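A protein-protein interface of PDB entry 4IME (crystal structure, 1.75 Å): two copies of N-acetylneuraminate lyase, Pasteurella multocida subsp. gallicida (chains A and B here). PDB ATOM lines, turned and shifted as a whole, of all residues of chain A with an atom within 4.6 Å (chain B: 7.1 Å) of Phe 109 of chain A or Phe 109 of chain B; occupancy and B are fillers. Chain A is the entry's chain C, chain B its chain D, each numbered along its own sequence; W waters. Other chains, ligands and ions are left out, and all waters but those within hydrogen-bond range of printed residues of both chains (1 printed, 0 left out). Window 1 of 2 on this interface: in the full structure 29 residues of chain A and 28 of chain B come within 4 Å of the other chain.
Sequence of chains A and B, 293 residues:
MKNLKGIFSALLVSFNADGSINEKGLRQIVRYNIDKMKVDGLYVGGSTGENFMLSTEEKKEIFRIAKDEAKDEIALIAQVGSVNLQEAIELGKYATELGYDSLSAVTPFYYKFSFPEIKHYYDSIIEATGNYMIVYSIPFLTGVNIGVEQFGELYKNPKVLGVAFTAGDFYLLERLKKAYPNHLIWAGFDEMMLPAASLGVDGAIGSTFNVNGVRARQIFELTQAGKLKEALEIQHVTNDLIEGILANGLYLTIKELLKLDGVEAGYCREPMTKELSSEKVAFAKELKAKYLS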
ATOM      1  N   PHE A  52     -11.005 -31.175 -35.756  1.00  0.00           N
ATOM      2  CA  PHE A  52     -11.581 -29.909 -35.321  1.00  0.00           C
ATOM      3  C   PHE A  52     -10.730 -28.676 -35.616  1.00  0.00           C
ATOM      4  O   PHE A  52     -11.216 -27.561 -35.498  1.00  0.00           O
ATOM      5  CB  PHE A  52     -12.041 -30.037 -33.855  1.00  0.00           C
ATOM      6  CG  PHE A  52     -13.076 -31.121 -33.700  1.00  0.00           C
ATOM      7  CD1 PHE A  52     -12.702 -32.410 -33.277  1.00  0.00           C
ATOM      8  CD2 PHE A  52     -14.387 -30.906 -34.133  1.00  0.00           C
ATOM      9  CE1 PHE A  52     -13.654 -33.447 -33.163  1.00  0.00           C
ATOM     10  CE2 PHE A  52     -15.352 -31.933 -34.009  1.00  0.00           C
ATOM     11  CZ  PHE A  52     -14.978 -33.201 -33.534  1.00  0.00           C
ATOM     12  N   VAL A  83     -19.578 -27.654 -33.961  1.00  0.00           N
ATOM     13  CA  VAL A  83     -20.474 -26.618 -33.389  1.00  0.00           C
ATOM     14  C   VAL A  83     -21.376 -26.049 -34.508  1.00  0.00           C
ATOM     15  O   VAL A  83     -22.464 -25.519 -34.242  1.00  0.00           O
ATOM     16  CB  VAL A  83     -19.612 -25.509 -32.725  1.00  0.00           C
ATOM     17  CG1 VAL A  83     -20.456 -24.513 -31.957  1.00  0.00           C
ATOM     18  CG2 VAL A  83     -18.629 -26.119 -31.740  1.00  0.00           C
ATOM     19  N   VAL A 106     -19.994 -35.799 -32.886  1.00  0.00           N
ATOM     20  CA  VAL A 106     -19.755 -35.325 -31.500  1.00  0.00           C
ATOM     21  C   VAL A 106     -20.946 -34.477 -30.990  1.00  0.00           C
ATOM     22  O   VAL A 106     -21.629 -33.751 -31.753  1.00  0.00           O
ATOM     23  CB  VAL A 106     -18.435 -34.544 -31.434  1.00  0.00           C
ATOM     24  CG1 VAL A 106     -18.446 -33.223 -32.196  1.00  0.00           C
ATOM     25  CG2 VAL A 106     -18.002 -34.297 -30.010  1.00  0.00           C
ATOM     26  N   THR A 107     -21.254 -34.571 -29.689  1.00  0.00           N
ATOM     27  CA  THR A 107     -22.131 -33.562 -29.128  1.00  0.00           C
ATOM     28  C   THR A 107     -21.627 -32.149 -29.374  1.00  0.00           C
ATOM     29  O   THR A 107     -20.438 -31.829 -29.163  1.00  0.00           O
ATOM     30  CB  THR A 107     -22.241 -33.709 -27.586  1.00  0.00           C
ATOM     31  OG1 THR A 107     -20.935 -33.616 -26.996  1.00  0.00           O
ATOM     32  CG2 THR A 107     -22.790 -35.057 -27.249  1.00  0.00           C
ATOM     33  N   PRO A 108     -22.527 -31.257 -29.780  1.00  0.00           N
ATOM     34  CA  PRO A 108     -22.057 -29.924 -30.050  1.00  0.00           C
ATOM     35  C   PRO A 108     -21.538 -29.291 -28.748  1.00  0.00           C
ATOM     36  O   PRO A 108     -22.059 -29.542 -27.613  1.00  0.00           O
ATOM     37  CB  PRO A 108     -23.287 -29.208 -30.621  1.00  0.00           C
ATOM     38  CG  PRO A 108     -24.427 -29.977 -30.055  1.00  0.00           C
ATOM     39  CD  PRO A 108     -23.965 -31.397 -29.999  1.00  0.00           C
ATOM     40  N   PHE A 109     -20.487 -28.519 -28.924  1.00  0.00           N
ATOM     41  CA  PHE A 109     -19.694 -28.053 -27.781  1.00  0.00           C
ATOM     42  C   PHE A 109     -19.464 -26.543 -27.827  1.00  0.00           C
ATOM     43  O   PHE A 109     -20.062 -25.835 -28.644  1.00  0.00           O
ATOM     44  CB  PHE A 109     -18.398 -28.883 -27.710  1.00  0.00           C
ATOM     45  CG  PHE A 109     -17.550 -28.845 -28.975  1.00  0.00           C
ATOM     46  CD1 PHE A 109     -16.604 -27.851 -29.150  1.00  0.00           C
ATOM     47  CD2 PHE A 109     -17.712 -29.805 -29.960  1.00  0.00           C
ATOM     48  CE1 PHE A 109     -15.834 -27.792 -30.296  1.00  0.00           C
ATOM     49  CE2 PHE A 109     -16.910 -29.778 -31.119  1.00  0.00           C
ATOM     50  CZ  PHE A 109     -16.003 -28.761 -31.301  1.00  0.00           C
ATOM     51  N   TYR A 110     -18.602 -26.045 -26.937  1.00  0.00           N
ATOM     52  CA  TYR A 110     -18.316 -24.614 -26.743  1.00  0.00           C
ATOM     53  C   TYR A 110     -19.523 -23.984 -26.079  1.00  0.00           C
ATOM     54  O   TYR A 110     -19.477 -23.768 -24.859  1.00  0.00           O
ATOM     55  CB  TYR A 110     -17.870 -23.855 -28.042  1.00  0.00           C
ATOM     56  CG  TYR A 110     -17.428 -22.445 -27.743  1.00  0.00           C
ATOM     57  CD1 TYR A 110     -16.168 -22.186 -27.186  1.00  0.00           C
ATOM     58  CD2 TYR A 110     -18.329 -21.360 -27.851  1.00  0.00           C
ATOM     59  CE1 TYR A 110     -15.766 -20.884 -26.849  1.00  0.00           C
ATOM     60  CE2 TYR A 110     -17.941 -20.063 -27.507  1.00  0.00           C
ATOM     61  CZ  TYR A 110     -16.671 -19.837 -27.010  1.00  0.00           C
ATOM     62  OH  TYR A 110     -16.261 -18.567 -26.712  1.00  0.00           O
ATOM     63  N   TYR A 111     -20.572 -23.665 -26.824  1.00  0.00           N
ATOM     64  CA  TYR A 111     -21.795 -23.182 -26.129  1.00  0.00           C
ATOM     65  C   TYR A 111     -22.385 -24.277 -25.253  1.00  0.00           C
ATOM     66  O   TYR A 111     -22.196 -25.446 -25.527  1.00  0.00           O
ATOM     67  CB  TYR A 111     -22.832 -22.751 -27.169  1.00  0.00           C
ATOM     68  CG  TYR A 111     -22.368 -21.614 -28.005  1.00  0.00           C
ATOM     69  CD1 TYR A 111     -22.007 -21.826 -29.330  1.00  0.00           C
ATOM     70  CD2 TYR A 111     -22.278 -20.304 -27.484  1.00  0.00           C
ATOM     71  CE1 TYR A 111     -21.633 -20.757 -30.137  1.00  0.00           C
ATOM     72  CE2 TYR A 111     -21.890 -19.221 -28.312  1.00  0.00           C
ATOM     73  CZ  TYR A 111     -21.545 -19.481 -29.610  1.00  0.00           C
ATOM     74  OH  TYR A 111     -21.165 -18.409 -30.375  1.00  0.00           O
ATOM     75  N   PHE A 113     -25.236 -26.047 -24.828  1.00  0.00           N
ATOM     76  CA  PHE A 113     -26.506 -26.408 -25.471  1.00  0.00           C
ATOM     77  C   PHE A 113     -27.335 -27.246 -24.513  1.00  0.00           C
ATOM     78  O   PHE A 113     -26.806 -28.095 -23.759  1.00  0.00           O
ATOM     79  CB  PHE A 113     -26.244 -27.213 -26.765  1.00  0.00           C
ATOM     80  CG  PHE A 113     -25.522 -26.433 -27.826  1.00  0.00           C
ATOM     81  CD1 PHE A 113     -24.159 -26.660 -28.096  1.00  0.00           C
ATOM     82  CD2 PHE A 113     -26.215 -25.466 -28.563  1.00  0.00           C
ATOM     83  CE1 PHE A 113     -23.530 -25.947 -29.090  1.00  0.00           C
ATOM     84  CE2 PHE A 113     -25.582 -24.746 -29.553  1.00  0.00           C
ATOM     85  CZ  PHE A 113     -24.233 -24.982 -29.805  1.00  0.00           C
ATOM     86  N   THR A 142     -15.710 -32.175 -24.256  1.00  0.00           N
ATOM     87  CA  THR A 142     -16.891 -31.302 -24.514  1.00  0.00           C
ATOM     88  C   THR A 142     -17.543 -30.778 -23.233  1.00  0.00           C
ATOM     89  O   THR A 142     -18.240 -29.788 -23.262  1.00  0.00           O
ATOM     90  CB  THR A 142     -17.999 -32.095 -25.246  1.00  0.00           C
ATOM     91  OG1 THR A 142     -18.442 -33.131 -24.394  1.00  0.00           O
ATOM     92  CG2 THR A 142     -17.487 -32.719 -26.548  1.00  0.00           C
ATOM     93  N   PHE B  52     -19.298 -19.150 -33.395  1.00  0.00           N
ATOM     94  CA  PHE B  52     -18.678 -20.477 -33.463  1.00  0.00           C
ATOM     95  C   PHE B  52     -19.577 -21.524 -34.129  1.00  0.00           C
ATOM     96  O   PHE B  52     -19.147 -22.645 -34.389  1.00  0.00           O
ATOM     97  CB  PHE B  52     -18.189 -20.877 -32.036  1.00  0.00           C
ATOM     98  CG  PHE B  52     -17.146 -19.925 -31.513  1.00  0.00           C
ATOM     99  CD1 PHE B  52     -17.467 -18.928 -30.582  1.00  0.00           C
ATOM    100  CD2 PHE B  52     -15.820 -19.964 -32.032  1.00  0.00           C
ATOM    101  CE1 PHE B  52     -16.504 -18.016 -30.155  1.00  0.00           C
ATOM    102  CE2 PHE B  52     -14.855 -19.072 -31.579  1.00  0.00           C
ATOM    103  CZ  PHE B  52     -15.187 -18.075 -30.650  1.00  0.00           C
ATOM    104  N   MET B  53     -20.816 -21.139 -34.430  1.00  0.00           N
ATOM    105  CA  MET B  53     -21.730 -21.975 -35.209  1.00  0.00           C
ATOM    106  C   MET B  53     -21.715 -21.688 -36.721  1.00  0.00           C
ATOM    107  O   MET B  53     -22.484 -22.309 -37.474  1.00  0.00           O
ATOM    108  CB  MET B  53     -23.142 -21.807 -34.666  1.00  0.00           C
ATOM    109  CG  MET B  53     -23.279 -22.384 -33.258  1.00  0.00           C
ATOM    110  SD  MET B  53     -24.993 -22.190 -32.631  1.00  0.00           S
ATOM    111  CE  MET B  53     -25.087 -20.443 -32.416  1.00  0.00           C
ATOM    112  N   GLY B  81     -10.660 -15.763 -33.585  1.00  0.00           N
ATOM    113  CA  GLY B  81     -10.178 -17.023 -33.029  1.00  0.00           C
ATOM    114  C   GLY B  81     -11.085 -18.228 -33.267  1.00  0.00           C
ATOM    115  O   GLY B  81     -12.288 -18.071 -33.555  1.00  0.00           O
ATOM    116  N   SER B  82     -10.514 -19.428 -33.105  1.00  0.00           N
ATOM    117  CA  SER B  82     -11.130 -20.649 -33.542  1.00  0.00           C
ATOM    118  C   SER B  82     -10.198 -21.783 -33.068  1.00  0.00           C
ATOM    119  O   SER B  82      -9.040 -21.556 -32.702  1.00  0.00           O
ATOM    120  CB  SER B  82     -11.089 -20.588 -35.089  1.00  0.00           C
ATOM    121  OG  SER B  82     -11.426 -21.736 -35.749  1.00  0.00           O
ATOM    122  N   VAL B  83     -10.696 -23.009 -33.126  1.00  0.00           N
ATOM    123  CA  VAL B  83      -9.792 -24.160 -33.025  1.00  0.00           C
ATOM    124  C   VAL B  83      -8.906 -24.279 -34.267  1.00  0.00           C
ATOM    125  O   VAL B  83      -7.829 -24.863 -34.202  1.00  0.00           O
ATOM    126  CB  VAL B  83     -10.620 -25.447 -32.822  1.00  0.00           C
ATOM    127  CG1 VAL B  83      -9.731 -26.642 -32.526  1.00  0.00           C
ATOM    128  CG2 VAL B  83     -11.602 -25.314 -31.653  1.00  0.00           C
ATOM    129  N   ASN B  84      -9.383 -23.754 -35.394  1.00  0.00           N
ATOM    130  CA  ASN B  84      -8.642 -23.769 -36.668  1.00  0.00           C
ATOM    131  C   ASN B  84      -7.807 -22.497 -36.777  1.00  0.00           C
ATOM    132  O   ASN B  84      -8.327 -21.434 -37.125  1.00  0.00           O
ATOM    133  CB  ASN B  84      -9.683 -23.859 -37.794  1.00  0.00           C
ATOM    134  CG  ASN B  84      -9.082 -23.965 -39.188  1.00  0.00           C
ATOM    135  OD1 ASN B  84      -9.801 -24.282 -40.193  1.00  0.00           O
ATOM    136  ND2 ASN B  84      -7.821 -23.742 -39.301  1.00  0.00           N
ATOM    137  N   VAL B 106     -10.178 -15.862 -29.156  1.00  0.00           N
ATOM    138  CA  VAL B 106     -10.449 -16.793 -28.039  1.00  0.00           C
ATOM    139  C   VAL B 106      -9.241 -17.751 -27.961  1.00  0.00           C
ATOM    140  O   VAL B 106      -8.624 -18.103 -28.990  1.00  0.00           O
ATOM    141  CB  VAL B 106     -11.771 -17.553 -28.290  1.00  0.00           C
ATOM    142  CG1 VAL B 106     -11.711 -18.466 -29.536  1.00  0.00           C
ATOM    143  CG2 VAL B 106     -12.232 -18.281 -27.017  1.00  0.00           C
ATOM    144  N   THR B 107      -8.901 -18.144 -26.751  1.00  0.00           N
ATOM    145  CA  THR B 107      -7.941 -19.276 -26.573  1.00  0.00           C
ATOM    146  C   THR B 107      -8.456 -20.482 -27.366  1.00  0.00           C
ATOM    147  O   THR B 107      -9.652 -20.780 -27.298  1.00  0.00           O
ATOM    148  CB  THR B 107      -7.837 -19.638 -25.105  1.00  0.00           C
ATOM    149  OG1 THR B 107      -9.129 -20.025 -24.599  1.00  0.00           O
ATOM    150  CG2 THR B 107      -7.381 -18.446 -24.337  1.00  0.00           C
ATOM    151  N   PRO B 108      -7.601 -21.186 -28.127  1.00  0.00           N
ATOM    152  CA  PRO B 108      -8.101 -22.386 -28.832  1.00  0.00           C
ATOM    153  C   PRO B 108      -8.594 -23.445 -27.825  1.00  0.00           C
ATOM    154  O   PRO B 108      -8.050 -23.586 -26.720  1.00  0.00           O
ATOM    155  CB  PRO B 108      -6.888 -22.875 -29.672  1.00  0.00           C
ATOM    156  CG  PRO B 108      -5.718 -22.291 -28.987  1.00  0.00           C
ATOM    157  CD  PRO B 108      -6.164 -20.994 -28.311  1.00  0.00           C
ATOM    158  N   PHE B 109      -9.687 -24.095 -28.187  1.00  0.00           N
ATOM    159  CA  PHE B 109     -10.445 -24.911 -27.272  1.00  0.00           C
ATOM    160  C   PHE B 109     -10.679 -26.292 -27.890  1.00  0.00           C
ATOM    161  O   PHE B 109     -10.004 -26.644 -28.887  1.00  0.00           O
ATOM    162  CB  PHE B 109     -11.750 -24.168 -26.890  1.00  0.00           C
ATOM    163  CG  PHE B 109     -12.588 -23.742 -28.058  1.00  0.00           C
ATOM    164  CD1 PHE B 109     -13.577 -24.561 -28.561  1.00  0.00           C
ATOM    165  CD2 PHE B 109     -12.417 -22.513 -28.604  1.00  0.00           C
ATOM    166  CE1 PHE B 109     -14.384 -24.155 -29.642  1.00  0.00           C
ATOM    167  CE2 PHE B 109     -13.180 -22.094 -29.709  1.00  0.00           C
ATOM    168  CZ  PHE B 109     -14.165 -22.921 -30.242  1.00  0.00           C
ATOM    169  N   TYR B 110     -11.554 -27.085 -27.249  1.00  0.00           N
ATOM    170  CA  TYR B 110     -11.800 -28.515 -27.558  1.00  0.00           C
ATOM    171  C   TYR B 110     -10.620 -29.388 -27.126  1.00  0.00           C
ATOM    172  O   TYR B 110     -10.630 -30.049 -26.096  1.00  0.00           O
ATOM    173  CB  TYR B 110     -12.157 -28.772 -29.038  1.00  0.00           C
ATOM    174  CG  TYR B 110     -12.676 -30.176 -29.230  1.00  0.00           C
ATOM    175  CD1 TYR B 110     -13.948 -30.551 -28.807  1.00  0.00           C
ATOM    176  CD2 TYR B 110     -11.873 -31.158 -29.764  1.00  0.00           C
ATOM    177  CE1 TYR B 110     -14.401 -31.854 -28.953  1.00  0.00           C
ATOM    178  CE2 TYR B 110     -12.313 -32.456 -29.928  1.00  0.00           C
ATOM    179  CZ  TYR B 110     -13.592 -32.810 -29.511  1.00  0.00           C
ATOM    180  OH  TYR B 110     -13.963 -34.121 -29.691  1.00  0.00           O
ATOM    181  N   TYR B 111      -9.579 -29.385 -27.937  1.00  0.00           N
ATOM    182  CA  TYR B 111      -8.359 -30.069 -27.534  1.00  0.00           C
ATOM    183  C   TYR B 111      -7.740 -29.361 -26.378  1.00  0.00           C
ATOM    184  O   TYR B 111      -7.959 -28.146 -26.228  1.00  0.00           O
ATOM    185  CB  TYR B 111      -7.327 -30.106 -28.689  1.00  0.00           C
ATOM    186  CG  TYR B 111      -7.846 -30.865 -29.891  1.00  0.00           C
ATOM    187  CD1 TYR B 111      -8.231 -30.201 -31.051  1.00  0.00           C
ATOM    188  CD2 TYR B 111      -7.907 -32.244 -29.880  1.00  0.00           C
ATOM    189  CE1 TYR B 111      -8.674 -30.914 -32.170  1.00  0.00           C
ATOM    190  CE2 TYR B 111      -8.388 -32.956 -30.985  1.00  0.00           C
ATOM    191  CZ  TYR B 111      -8.770 -32.291 -32.129  1.00  0.00           C
ATOM    192  OH  TYR B 111      -9.214 -33.066 -33.231  1.00  0.00           O
ATOM    193  N   LYS B 112      -6.944 -30.109 -25.587  1.00  0.00           N
ATOM    194  CA  LYS B 112      -6.312 -29.504 -24.373  1.00  0.00           C
ATOM    195  C   LYS B 112      -4.921 -28.969 -24.761  1.00  0.00           C
ATOM    196  O   LYS B 112      -3.881 -29.564 -24.415  1.00  0.00           O
ATOM    197  CB  LYS B 112      -6.212 -30.509 -23.205  1.00  0.00           C
ATOM    198  CG  LYS B 112      -7.564 -31.100 -22.780  1.00  0.00           C
ATOM    199  CD  LYS B 112      -8.573 -30.027 -22.420  1.00  0.00           C
ATOM    200  CE  LYS B 112      -9.677 -30.530 -21.466  1.00  0.00           C
ATOM    201  NZ  LYS B 112     -10.663 -29.431 -21.308  1.00  0.00           N
ATOM    202  N   PHE B 113      -4.905 -27.862 -25.507  1.00  0.00           N
ATOM    203  CA  PHE B 113      -3.628 -27.276 -25.959  1.00  0.00           C
ATOM    204  C   PHE B 113      -2.762 -26.846 -24.761  1.00  0.00           C
ATOM    205  O   PHE B 113      -3.274 -26.328 -23.754  1.00  0.00           O
ATOM    206  CB  PHE B 113      -3.913 -26.060 -26.870  1.00  0.00           C
ATOM    207  CG  PHE B 113      -4.636 -26.417 -28.140  1.00  0.00           C
ATOM    208  CD1 PHE B 113      -5.991 -26.142 -28.304  1.00  0.00           C
ATOM    209  CD2 PHE B 113      -3.947 -27.010 -29.195  1.00  0.00           C
ATOM    210  CE1 PHE B 113      -6.649 -26.448 -29.486  1.00  0.00           C
ATOM    211  CE2 PHE B 113      -4.617 -27.348 -30.381  1.00  0.00           C
ATOM    212  CZ  PHE B 113      -5.967 -27.067 -30.528  1.00  0.00           C
ATOM    213  N   TYR B 121      -0.141 -19.777 -31.140  1.00  0.00           N
ATOM    214  CA  TYR B 121      -1.371 -19.423 -31.852  1.00  0.00           C
ATOM    215  C   TYR B 121      -1.559 -17.916 -31.873  1.00  0.00           C
ATOM    216  O   TYR B 121      -1.805 -17.347 -32.946  1.00  0.00           O
ATOM    217  CB  TYR B 121      -2.537 -20.106 -31.144  1.00  0.00           C
ATOM    218  CG  TYR B 121      -3.941 -19.632 -31.322  1.00  0.00           C
ATOM    219  CD1 TYR B 121      -4.822 -20.317 -32.167  1.00  0.00           C
ATOM    220  CD2 TYR B 121      -4.443 -18.592 -30.542  1.00  0.00           C
ATOM    221  CE1 TYR B 121      -6.164 -19.934 -32.317  1.00  0.00           C
ATOM    222  CE2 TYR B 121      -5.800 -18.231 -30.632  1.00  0.00           C
ATOM    223  CZ  TYR B 121      -6.656 -18.895 -31.489  1.00  0.00           C
ATOM    224  OH  TYR B 121      -8.008 -18.553 -31.560  1.00  0.00           O
ATOM    225  N   LEU B 141     -16.464 -21.386 -20.762  1.00  0.00           N
ATOM    226  CA  LEU B 141     -16.767 -22.131 -22.022  1.00  0.00           C
ATOM    227  C   LEU B 141     -15.593 -22.927 -22.556  1.00  0.00           C
ATOM    228  O   LEU B 141     -15.799 -23.999 -23.151  1.00  0.00           O
ATOM    229  CB  LEU B 141     -17.297 -21.211 -23.128  1.00  0.00           C
ATOM    230  CG  LEU B 141     -18.536 -20.358 -22.822  1.00  0.00           C
ATOM    231  CD1 LEU B 141     -18.983 -19.576 -24.056  1.00  0.00           C
ATOM    232  CD2 LEU B 141     -19.667 -21.262 -22.313  1.00  0.00           C
ATOM    233  N   THR B 142     -14.374 -22.395 -22.411  1.00  0.00           N
ATOM    234  CA  THR B 142     -13.209 -23.046 -23.039  1.00  0.00           C
ATOM    235  C   THR B 142     -12.542 -24.045 -22.096  1.00  0.00           C
ATOM    236  O   THR B 142     -11.922 -24.992 -22.550  1.00  0.00           O
ATOM    237  CB  THR B 142     -12.131 -22.045 -23.436  1.00  0.00           C
ATOM    238  OG1 THR B 142     -11.618 -21.445 -22.249  1.00  0.00           O
ATOM    239  CG2 THR B 142     -12.600 -20.976 -24.476  1.00  0.00           C
ATOM    240  N   GLY B 143     -12.653 -23.824 -20.777  1.00  0.00           N
ATOM    241  CA  GLY B 143     -11.895 -24.670 -19.812  1.00  0.00           C
ATOM    242  C   GLY B 143     -10.418 -24.272 -19.742  1.00  0.00           C
ATOM    243  O   GLY B 143      -9.611 -24.944 -19.078  1.00  0.00           O
ATOM    244  N   VAL B 144     -10.045 -23.190 -20.408  1.00  0.00           N
ATOM    245  CA  VAL B 144      -8.638 -22.750 -20.396  1.00  0.00           C
ATOM    246  C   VAL B 144      -8.424 -21.677 -19.311  1.00  0.00           C
ATOM    247  O   VAL B 144      -9.141 -20.696 -19.257  1.00  0.00           O
ATOM    248  CB  VAL B 144      -8.255 -22.171 -21.766  1.00  0.00           C
ATOM    249  CG1 VAL B 144      -6.837 -21.605 -21.777  1.00  0.00           C
ATOM    250  CG2 VAL B 144      -8.384 -23.277 -22.813  1.00  0.00           C
ATOM    251  N   PRO B 271     -27.360 -24.908 -34.004  1.00  0.00           N
ATOM    252  CA  PRO B 271     -28.159 -25.669 -33.035  1.00  0.00           C
ATOM    253  C   PRO B 271     -28.707 -24.938 -31.819  1.00  0.00           C
ATOM    254  O   PRO B 271     -29.420 -25.575 -31.010  1.00  0.00           O
ATOM    255  CB  PRO B 271     -27.215 -26.789 -32.597  1.00  0.00           C
ATOM    256  CG  PRO B 271     -25.822 -26.273 -32.854  1.00  0.00           C
ATOM    257  CD  PRO B 271     -25.929 -25.308 -33.987  1.00  0.00           C
HETATM  258  O   HOH W   1     -18.051 -25.276 -23.013  1.00  0.00           O
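The side-chain hydroxyl (OG1) of Thr 142 of chain B sits at hydrogen-bond distance from the backbone NH (N) of Val 144 of chain B, 3.0 Å away.
Among the printed residues, merely in contact across the chains: Tyr 110 of chain A with Phe 52 of chain B, Val 83 of chain A with Phe 52 of chain B, Phe 52 of chain A with Tyr 110 of chain B, Val 83 of chain A with Met 53 of chain B, Phe 52 of chain A with Val 83 of chain B, Val 83 of chain A with Pro 271 of chain B, Phe 52 of chain A with Tyr 111 of chain B, Tyr 110 of chain A with Leu 141 of chain B, Tyr 110 of chain A with Phe 109 of chain B, Tyr 111 of chain A with Phe 52 of chain B, Phe 113 of chain A with Pro 271 of chain B, Phe 109 of chain A with Tyr 110 of chain B, Tyr 111 of chain A with Met 53 of chain B, Tyr 110 of chain A with Thr 142 of chain B and Phe 109 of chain A with Phe 109 of chain B.
Of chain B, only Phe 109 and Tyr 110 come within 4 Å of Phe 109 of chain A. Phe 109 of chain B touches just these residues of chain A: Phe 109 (3.97 Å) and Tyr 110 (3.6 Å). Of the printed residues of chain A, Pro 271 of chain B touches Val 83 and Phe 113. Of the printed residues of chain A, Tyr 110 of chain B touches Phe 52 and Phe 109. Of the printed residues of chain A, Phe 52 of chain B touches Val 83 (3.3 Å), Tyr 110 (3.3 Å) and Tyr 111 (3.6 Å). Of the printed residues of chain A, Thr 142 of chain B touches Tyr 110 (3.96 Å). The nearest residue of chain B that does not touch Phe 109 of chain A is Val 83 of chain B (5.1 Å). The nearest printed residue of chain A that does not touch Phe 109 of chain B is Val 83 of chain A (5.1 Å). The nearest printed residue of chain A that does not touch Met 53 of chain B is Phe 113 of chain A (4.04 Å).
Printed residues of chain A that touch a printed residue of chain B: Phe 52, Val 83, Phe 109, Tyr 110, Tyr 111 and Phe 113. Of the 20 printed residues of chain B, 9 touch a printed residue of chain A. Printed residues of chain B that touch a printed residue of chain A: Phe 52, Met 53, Val 83, Phe 109, Tyr 110, Tyr 111, Leu 141, Thr 142 and Pro 271. Among the printed residues, 15 pairs touch across the chains.
Phe 52 of chain A touches Tyr 110 of chain B, and with the chains exchanged Tyr 110 of chain A touches Phe 52 of chain B. Phe 52 of chain A touches Tyr 111 of chain B, and with the chains exchanged Tyr 111 of chain A touches Phe 52 of chain B. Phe 109 of chain B touches its own counterpart, Phe 109 of chain A. Phe 109 of chain A touches Tyr 110 of chain B, and with the chains exchanged Tyr 110 of chain A touches Phe 109 of chain B.
Water W1 lies within hydrogen-bond range of the backbone carbonyl oxygen (O) of Leu 141 of chain B (2.6 Å) and the backbone carbonyl oxygen (O) of Tyr 110 of chain A (2.8 Å).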
